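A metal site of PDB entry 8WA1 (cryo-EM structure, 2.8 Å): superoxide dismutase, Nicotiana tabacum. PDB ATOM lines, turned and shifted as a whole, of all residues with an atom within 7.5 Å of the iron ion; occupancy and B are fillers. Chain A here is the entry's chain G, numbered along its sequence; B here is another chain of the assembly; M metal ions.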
ATOM      1  N   HIS A  77      -7.360  -8.177   8.143  1.00  0.00           N
ATOM      2  CA  HIS A  77      -6.981  -9.098   9.195  1.00  0.00           C
ATOM      3  C   HIS A  77      -5.624  -8.719   9.741  1.00  0.00           C
ATOM      4  O   HIS A  77      -5.395  -8.769  10.933  1.00  0.00           O
ATOM      5  CB  HIS A  77      -6.949 -10.521   8.657  1.00  0.00           C
ATOM      6  CG  HIS A  77      -6.996 -11.580   9.716  1.00  0.00           C
ATOM      7  ND1 HIS A  77      -6.771 -12.903   9.440  1.00  0.00           N
ATOM      8  CD2 HIS A  77      -7.245 -11.498  11.046  1.00  0.00           C
ATOM      9  CE1 HIS A  77      -6.881 -13.609  10.558  1.00  0.00           C
ATOM     10  NE2 HIS A  77      -7.167 -12.772  11.548  1.00  0.00           N
ATOM     11  N   TRP A  78      -4.725  -8.335   8.866  1.00  0.00           N
ATOM     12  CA  TRP A  78      -3.404  -7.975   9.311  1.00  0.00           C
ATOM     13  C   TRP A  78      -3.388  -6.548   9.747  1.00  0.00           C
ATOM     14  O   TRP A  78      -3.125  -6.257  10.904  1.00  0.00           O
ATOM     15  CB  TRP A  78      -2.392  -8.169   8.186  1.00  0.00           C
ATOM     16  CG  TRP A  78      -0.985  -7.895   8.588  1.00  0.00           C
ATOM     17  CD1 TRP A  78      -0.250  -8.559   9.520  1.00  0.00           C
ATOM     18  CD2 TRP A  78      -0.134  -6.888   8.051  1.00  0.00           C
ATOM     19  NE1 TRP A  78       1.008  -8.019   9.605  1.00  0.00           N
ATOM     20  CE2 TRP A  78       1.100  -6.993   8.704  1.00  0.00           C
ATOM     21  CE3 TRP A  78      -0.297  -5.898   7.069  1.00  0.00           C
ATOM     22  CZ2 TRP A  78       2.178  -6.146   8.425  1.00  0.00           C
ATOM     23  CZ3 TRP A  78       0.762  -5.064   6.791  1.00  0.00           C
ATOM     24  CH2 TRP A  78       1.988  -5.194   7.463  1.00  0.00           C
ATOM     25  N   HIS A  81      -6.334  -6.150  12.811  1.00  0.00           N
ATOM     26  CA  HIS A  81      -6.303  -7.009  13.984  1.00  0.00           C
ATOM     27  C   HIS A  81      -4.922  -7.190  14.549  1.00  0.00           C
ATOM     28  O   HIS A  81      -4.706  -7.040  15.742  1.00  0.00           O
ATOM     29  CB  HIS A  81      -6.890  -8.367  13.643  1.00  0.00           C
ATOM     30  CG  HIS A  81      -8.328  -8.314  13.229  1.00  0.00           C
ATOM     31  ND1 HIS A  81      -9.354  -8.229  14.140  1.00  0.00           N
ATOM     32  CD2 HIS A  81      -8.905  -8.329  11.999  1.00  0.00           C
ATOM     33  CE1 HIS A  81     -10.501  -8.187  13.491  1.00  0.00           C
ATOM     34  NE2 HIS A  81     -10.261  -8.254  12.198  1.00  0.00           N
ATOM     35  N   HIS A  82      -3.960  -7.453  13.675  1.00  0.00           N
ATOM     36  CA  HIS A  82      -2.628  -7.711  14.160  1.00  0.00           C
ATOM     37  C   HIS A  82      -2.061  -6.468  14.823  1.00  0.00           C
ATOM     38  O   HIS A  82      -1.467  -6.542  15.894  1.00  0.00           O
ATOM     39  CB  HIS A  82      -1.736  -8.173  13.018  1.00  0.00           C
ATOM     40  CG  HIS A  82      -0.658  -9.113  13.428  1.00  0.00           C
ATOM     41  ND1 HIS A  82      -0.609 -10.420  13.001  1.00  0.00           N
ATOM     42  CD2 HIS A  82       0.432  -8.939  14.216  1.00  0.00           C
ATOM     43  CE1 HIS A  82       0.455 -11.012  13.516  1.00  0.00           C
ATOM     44  NE2 HIS A  82       1.101 -10.129  14.262  1.00  0.00           N
ATOM     45  N   TYR A  85      -3.388  -5.747  18.320  1.00  0.00           N
ATOM     46  CA  TYR A  85      -2.880  -6.527  19.422  1.00  0.00           C
ATOM     47  C   TYR A  85      -1.513  -6.060  19.878  1.00  0.00           C
ATOM     48  O   TYR A  85      -1.325  -5.776  21.063  1.00  0.00           O
ATOM     49  CB  TYR A  85      -2.821  -7.995  19.044  1.00  0.00           C
ATOM     50  CG  TYR A  85      -4.160  -8.647  18.807  1.00  0.00           C
ATOM     51  CD1 TYR A  85      -5.184  -8.533  19.741  1.00  0.00           C
ATOM     52  CD2 TYR A  85      -4.397  -9.391  17.671  1.00  0.00           C
ATOM     53  CE1 TYR A  85      -6.408  -9.130  19.521  1.00  0.00           C
ATOM     54  CE2 TYR A  85      -5.619  -9.991  17.442  1.00  0.00           C
ATOM     55  CZ  TYR A  85      -6.610  -9.861  18.376  1.00  0.00           C
ATOM     56  OH  TYR A  85      -7.834 -10.457  18.156  1.00  0.00           O
ATOM     57  N   GLN A 126      -2.598 -13.821  21.027  1.00  0.00           N
ATOM     58  CA  GLN A 126      -3.156 -13.507  19.731  1.00  0.00           C
ATOM     59  C   GLN A 126      -2.070 -13.075  18.783  1.00  0.00           C
ATOM     60  O   GLN A 126      -2.035 -13.535  17.660  1.00  0.00           O
ATOM     61  CB  GLN A 126      -4.266 -12.488  19.847  1.00  0.00           C
ATOM     62  CG  GLN A 126      -5.589 -13.080  20.303  1.00  0.00           C
ATOM     63  CD  GLN A 126      -6.233 -13.984  19.266  1.00  0.00           C
ATOM     64  OE1 GLN A 126      -6.000 -15.187  19.230  1.00  0.00           O
ATOM     65  NE2 GLN A 126      -7.074 -13.391  18.415  1.00  0.00           N
ATOM     66  N   ASN A 129      -0.178 -16.122  17.601  1.00  0.00           N
ATOM     67  CA  ASN A 129      -0.902 -17.025  16.744  1.00  0.00           C
ATOM     68  C   ASN A 129      -1.163 -16.452  15.379  1.00  0.00           C
ATOM     69  O   ASN A 129      -1.124 -17.153  14.393  1.00  0.00           O
ATOM     70  CB  ASN A 129      -2.088 -17.746  17.422  1.00  0.00           C
ATOM     71  CG  ASN A 129      -3.038 -16.825  18.143  1.00  0.00           C
ATOM     72  OD1 ASN A 129      -3.413 -17.093  19.277  1.00  0.00           O
ATOM     73  ND2 ASN A 129      -3.443 -15.756  17.490  1.00  0.00           N
ATOM     74  N   HIS A 130      -1.451 -15.163  15.308  1.00  0.00           N
ATOM     75  CA  HIS A 130      -1.659 -14.550  14.028  1.00  0.00           C
ATOM     76  C   HIS A 130      -0.387 -14.591  13.204  1.00  0.00           C
ATOM     77  O   HIS A 130      -0.411 -14.837  11.988  1.00  0.00           O
ATOM     78  CB  HIS A 130      -2.180 -13.129  14.189  1.00  0.00           C
ATOM     79  CG  HIS A 130      -3.655 -13.075  14.444  1.00  0.00           C
ATOM     80  ND1 HIS A 130      -4.183 -13.105  15.718  1.00  0.00           N
ATOM     81  CD2 HIS A 130      -4.708 -13.001  13.594  1.00  0.00           C
ATOM     82  CE1 HIS A 130      -5.502 -13.046  15.631  1.00  0.00           C
ATOM     83  NE2 HIS A 130      -5.846 -12.984  14.361  1.00  0.00           N
ATOM     84  N   PHE A 133      -0.005 -17.969  11.842  1.00  0.00           N
ATOM     85  CA  PHE A 133      -0.966 -18.190  10.771  1.00  0.00           C
ATOM     86  C   PHE A 133      -0.476 -17.604   9.476  1.00  0.00           C
ATOM     87  O   PHE A 133      -0.550 -18.232   8.420  1.00  0.00           O
ATOM     88  CB  PHE A 133      -2.246 -17.480  11.177  1.00  0.00           C
ATOM     89  CG  PHE A 133      -3.362 -17.605  10.206  1.00  0.00           C
ATOM     90  CD1 PHE A 133      -4.011 -18.810  10.029  1.00  0.00           C
ATOM     91  CD2 PHE A 133      -3.794 -16.502   9.487  1.00  0.00           C
ATOM     92  CE1 PHE A 133      -5.063 -18.927   9.137  1.00  0.00           C
ATOM     93  CE2 PHE A 133      -4.841 -16.611   8.593  1.00  0.00           C
ATOM     94  CZ  PHE A 133      -5.481 -17.820   8.420  1.00  0.00           C
ATOM     95  N   TRP A 134       0.056 -16.396   9.544  1.00  0.00           N
ATOM     96  CA  TRP A 134       0.589 -15.812   8.338  1.00  0.00           C
ATOM     97  C   TRP A 134       1.677 -16.696   7.747  1.00  0.00           C
ATOM     98  O   TRP A 134       1.679 -16.939   6.558  1.00  0.00           O
ATOM     99  CB  TRP A 134       1.111 -14.399   8.562  1.00  0.00           C
ATOM    100  CG  TRP A 134       0.096 -13.424   9.033  1.00  0.00           C
ATOM    101  CD1 TRP A 134       0.210 -12.579  10.096  1.00  0.00           C
ATOM    102  CD2 TRP A 134      -1.197 -13.196   8.481  1.00  0.00           C
ATOM    103  NE1 TRP A 134      -0.932 -11.834  10.233  1.00  0.00           N
ATOM    104  CE2 TRP A 134      -1.811 -12.198   9.254  1.00  0.00           C
ATOM    105  CE3 TRP A 134      -1.904 -13.729   7.393  1.00  0.00           C
ATOM    106  CZ2 TRP A 134      -3.091 -11.721   8.989  1.00  0.00           C
ATOM    107  CZ3 TRP A 134      -3.172 -13.268   7.139  1.00  0.00           C
ATOM    108  CH2 TRP A 134      -3.748 -12.277   7.924  1.00  0.00           C
ATOM    109  N   GLY A 178     -11.682 -19.614  17.836  1.00  0.00           N
ATOM    110  CA  GLY A 178     -10.604 -20.430  18.350  1.00  0.00           C
ATOM    111  C   GLY A 178      -9.613 -20.757  17.264  1.00  0.00           C
ATOM    112  O   GLY A 178      -9.640 -20.117  16.219  1.00  0.00           O
ATOM    113  N   TRP A 179      -8.714 -21.693  17.516  1.00  0.00           N
ATOM    114  CA  TRP A 179      -7.762 -22.108  16.503  1.00  0.00           C
ATOM    115  C   TRP A 179      -7.657 -23.630  16.549  1.00  0.00           C
ATOM    116  O   TRP A 179      -7.993 -24.229  17.565  1.00  0.00           O
ATOM    117  CB  TRP A 179      -6.405 -21.472  16.762  1.00  0.00           C
ATOM    118  CG  TRP A 179      -6.352 -19.975  16.711  1.00  0.00           C
ATOM    119  CD1 TRP A 179      -6.916 -19.097  17.591  1.00  0.00           C
ATOM    120  CD2 TRP A 179      -5.659 -19.180  15.746  1.00  0.00           C
ATOM    121  NE1 TRP A 179      -6.647 -17.805  17.213  1.00  0.00           N
ATOM    122  CE2 TRP A 179      -5.867 -17.838  16.084  1.00  0.00           C
ATOM    123  CE3 TRP A 179      -4.891 -19.479  14.626  1.00  0.00           C
ATOM    124  CZ2 TRP A 179      -5.335 -16.792  15.341  1.00  0.00           C
ATOM    125  CZ3 TRP A 179      -4.369 -18.450  13.887  1.00  0.00           C
ATOM    126  CH2 TRP A 179      -4.589 -17.121  14.240  1.00  0.00           C
ATOM    127  N   ASP A 214      -7.053 -19.981  11.782  1.00  0.00           N
ATOM    128  CA  ASP A 214      -7.861 -19.058  12.561  1.00  0.00           C
ATOM    129  C   ASP A 214      -9.319 -19.363  12.371  1.00  0.00           C
ATOM    130  O   ASP A 214      -9.835 -19.261  11.264  1.00  0.00           O
ATOM    131  CB  ASP A 214      -7.588 -17.618  12.121  1.00  0.00           C
ATOM    132  CG  ASP A 214      -8.027 -16.606  13.154  1.00  0.00           C
ATOM    133  OD1 ASP A 214      -8.552 -17.022  14.202  1.00  0.00           O
ATOM    134  OD2 ASP A 214      -7.839 -15.390  12.932  1.00  0.00           O
ATOM    135  N   LEU A 215      -9.983 -19.735  13.454  1.00  0.00           N
ATOM    136  CA  LEU A 215     -11.402 -19.993  13.388  1.00  0.00           C
ATOM    137  C   LEU A 215     -12.148 -18.812  13.928  1.00  0.00           C
ATOM    138  O   LEU A 215     -13.370 -18.855  14.076  1.00  0.00           O
ATOM    139  CB  LEU A 215     -11.781 -21.260  14.141  1.00  0.00           C
ATOM    140  CG  LEU A 215     -11.241 -22.542  13.525  1.00  0.00           C
ATOM    141  CD1 LEU A 215     -11.754 -23.747  14.296  1.00  0.00           C
ATOM    142  CD2 LEU A 215     -11.669 -22.637  12.066  1.00  0.00           C
ATOM    143  N   TRP A 216     -11.435 -17.745  14.268  1.00  0.00           N
ATOM    144  CA  TRP A 216     -12.139 -16.556  14.670  1.00  0.00           C
ATOM    145  C   TRP A 216     -12.838 -16.059  13.428  1.00  0.00           C
ATOM    146  O   TRP A 216     -12.294 -16.135  12.326  1.00  0.00           O
ATOM    147  CB  TRP A 216     -11.185 -15.501  15.231  1.00  0.00           C
ATOM    148  CG  TRP A 216     -10.711 -15.775  16.623  1.00  0.00           C
ATOM    149  CD1 TRP A 216     -10.097 -16.907  17.065  1.00  0.00           C
ATOM    150  CD2 TRP A 216     -10.788 -14.887  17.732  1.00  0.00           C
ATOM    151  NE1 TRP A 216      -9.800 -16.779  18.399  1.00  0.00           N
ATOM    152  CE2 TRP A 216     -10.214 -15.551  18.835  1.00  0.00           C
ATOM    153  CE3 TRP A 216     -11.298 -13.597  17.918  1.00  0.00           C
ATOM    154  CZ2 TRP A 216     -10.123 -14.973  20.095  1.00  0.00           C
ATOM    155  CZ3 TRP A 216     -11.206 -13.023  19.168  1.00  0.00           C
ATOM    156  CH2 TRP A 216     -10.630 -13.707  20.247  1.00  0.00           C
ATOM    157  N   GLU A 217     -14.051 -15.533  13.572  1.00  0.00           N
ATOM    158  CA  GLU A 217     -14.833 -15.130  12.416  1.00  0.00           C
ATOM    159  C   GLU A 217     -14.226 -14.015  11.606  1.00  0.00           C
ATOM    160  O   GLU A 217     -14.442 -13.953  10.401  1.00  0.00           O
ATOM    161  CB  GLU A 217     -16.251 -14.756  12.829  1.00  0.00           C
ATOM    162  CG  GLU A 217     -16.958 -15.820  13.648  1.00  0.00           C
ATOM    163  CD  GLU A 217     -18.374 -15.436  14.013  1.00  0.00           C
ATOM    164  OE1 GLU A 217     -18.811 -14.326  13.658  1.00  0.00           O
ATOM    165  OE2 GLU A 217     -19.058 -16.263  14.660  1.00  0.00           O
ATOM    166  N   HIS A 218     -13.447 -13.159  12.240  1.00  0.00           N
ATOM    167  CA  HIS A 218     -12.931 -12.024  11.522  1.00  0.00           C
ATOM    168  C   HIS A 218     -12.125 -12.484  10.335  1.00  0.00           C
ATOM    169  O   HIS A 218     -12.068 -11.814   9.320  1.00  0.00           O
ATOM    170  CB  HIS A 218     -12.111 -11.079  12.396  1.00  0.00           C
ATOM    171  CG  HIS A 218     -11.050 -11.740  13.218  1.00  0.00           C
ATOM    172  ND1 HIS A 218     -10.945 -11.561  14.583  1.00  0.00           N
ATOM    173  CD2 HIS A 218     -10.020 -12.555  12.884  1.00  0.00           C
ATOM    174  CE1 HIS A 218      -9.914 -12.242  15.050  1.00  0.00           C
ATOM    175  NE2 HIS A 218      -9.338 -12.854  14.027  1.00  0.00           N
ATOM    176  N   ALA A 219     -11.493 -13.631  10.454  1.00  0.00           N
ATOM    177  CA  ALA A 219     -10.748 -14.164   9.350  1.00  0.00           C
ATOM    178  C   ALA A 219     -11.592 -14.484   8.127  1.00  0.00           C
ATOM    179  O   ALA A 219     -11.196 -14.175   7.015  1.00  0.00           O
ATOM    180  CB  ALA A 219     -10.016 -15.403   9.789  1.00  0.00           C
ATOM    181  N   TYR A 220     -12.751 -15.102   8.323  1.00  0.00           N
ATOM    182  CA  TYR A 220     -13.509 -15.544   7.151  1.00  0.00           C
ATOM    183  C   TYR A 220     -14.790 -14.829   6.741  1.00  0.00           C
ATOM    184  O   TYR A 220     -15.216 -14.994   5.602  1.00  0.00           O
ATOM    185  CB  TYR A 220     -13.800 -17.040   7.254  1.00  0.00           C
ATOM    186  CG  TYR A 220     -14.639 -17.444   8.452  1.00  0.00           C
ATOM    187  CD1 TYR A 220     -16.022 -17.383   8.405  1.00  0.00           C
ATOM    188  CD2 TYR A 220     -14.050 -17.897   9.614  1.00  0.00           C
ATOM    189  CE1 TYR A 220     -16.786 -17.745   9.481  1.00  0.00           C
ATOM    190  CE2 TYR A 220     -14.811 -18.271  10.697  1.00  0.00           C
ATOM    191  CZ  TYR A 220     -16.175 -18.193  10.625  1.00  0.00           C
ATOM    192  OH  TYR A 220     -16.944 -18.563  11.703  1.00  0.00           O
ATOM    193  N   GLU B 227     -19.000 -11.388  16.067  1.00  0.00           N
ATOM    194  CA  GLU B 227     -18.550 -10.691  14.871  1.00  0.00           C
ATOM    195  C   GLU B 227     -19.621 -10.564  13.827  1.00  0.00           C
ATOM    196  O   GLU B 227     -19.727  -9.541  13.178  1.00  0.00           O
ATOM    197  CB  GLU B 227     -17.308 -11.364  14.296  1.00  0.00           C
ATOM    198  CG  GLU B 227     -15.999 -10.777  14.797  1.00  0.00           C
ATOM    199  CD  GLU B 227     -15.006 -11.846  15.206  1.00  0.00           C
ATOM    200  OE1 GLU B 227     -15.417 -12.998  15.435  1.00  0.00           O
ATOM    201  OE2 GLU B 227     -13.792 -11.524  15.317  1.00  0.00           O
HETATM  202 FE    FE M   1      -7.396 -13.644  13.285  1.00  0.00          FE
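The iron ion is bound by OD2 of Asp 214, at 1.8 Å.
The iron ion is bound by NE2 of His 77, at 2.0 Å.
NE2 of His 130 is bound to the iron ion (2.0 Å).
A ring nitrogen (NE2) of His 218 is bound to the iron ion (2.2 Å).
Four residues have an atom within 4 Å of the iron ion: His 77, His 130, Asp 214 and His 218.
The side-chain carboxylate (OD1) of Asp 214 is in hydrogen-bond range of the backbone NH (N) of Trp 216 (3.0 Å).
O of His 77 is in hydrogen-bond range of N of His 82.
ND1 of His 130 is in hydrogen-bond range of O of Gln 126, 2.9 Å away.
A ring nitrogen (ND1) of His 130 is in hydrogen-bond range of the side-chain amide nitrogen (ND2) of Asn 129.
A ring nitrogen (ND1) of His 218 is in hydrogen-bond range of the side-chain carboxylate (OE2) of Glu 227 of chain B (2.9 Å).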
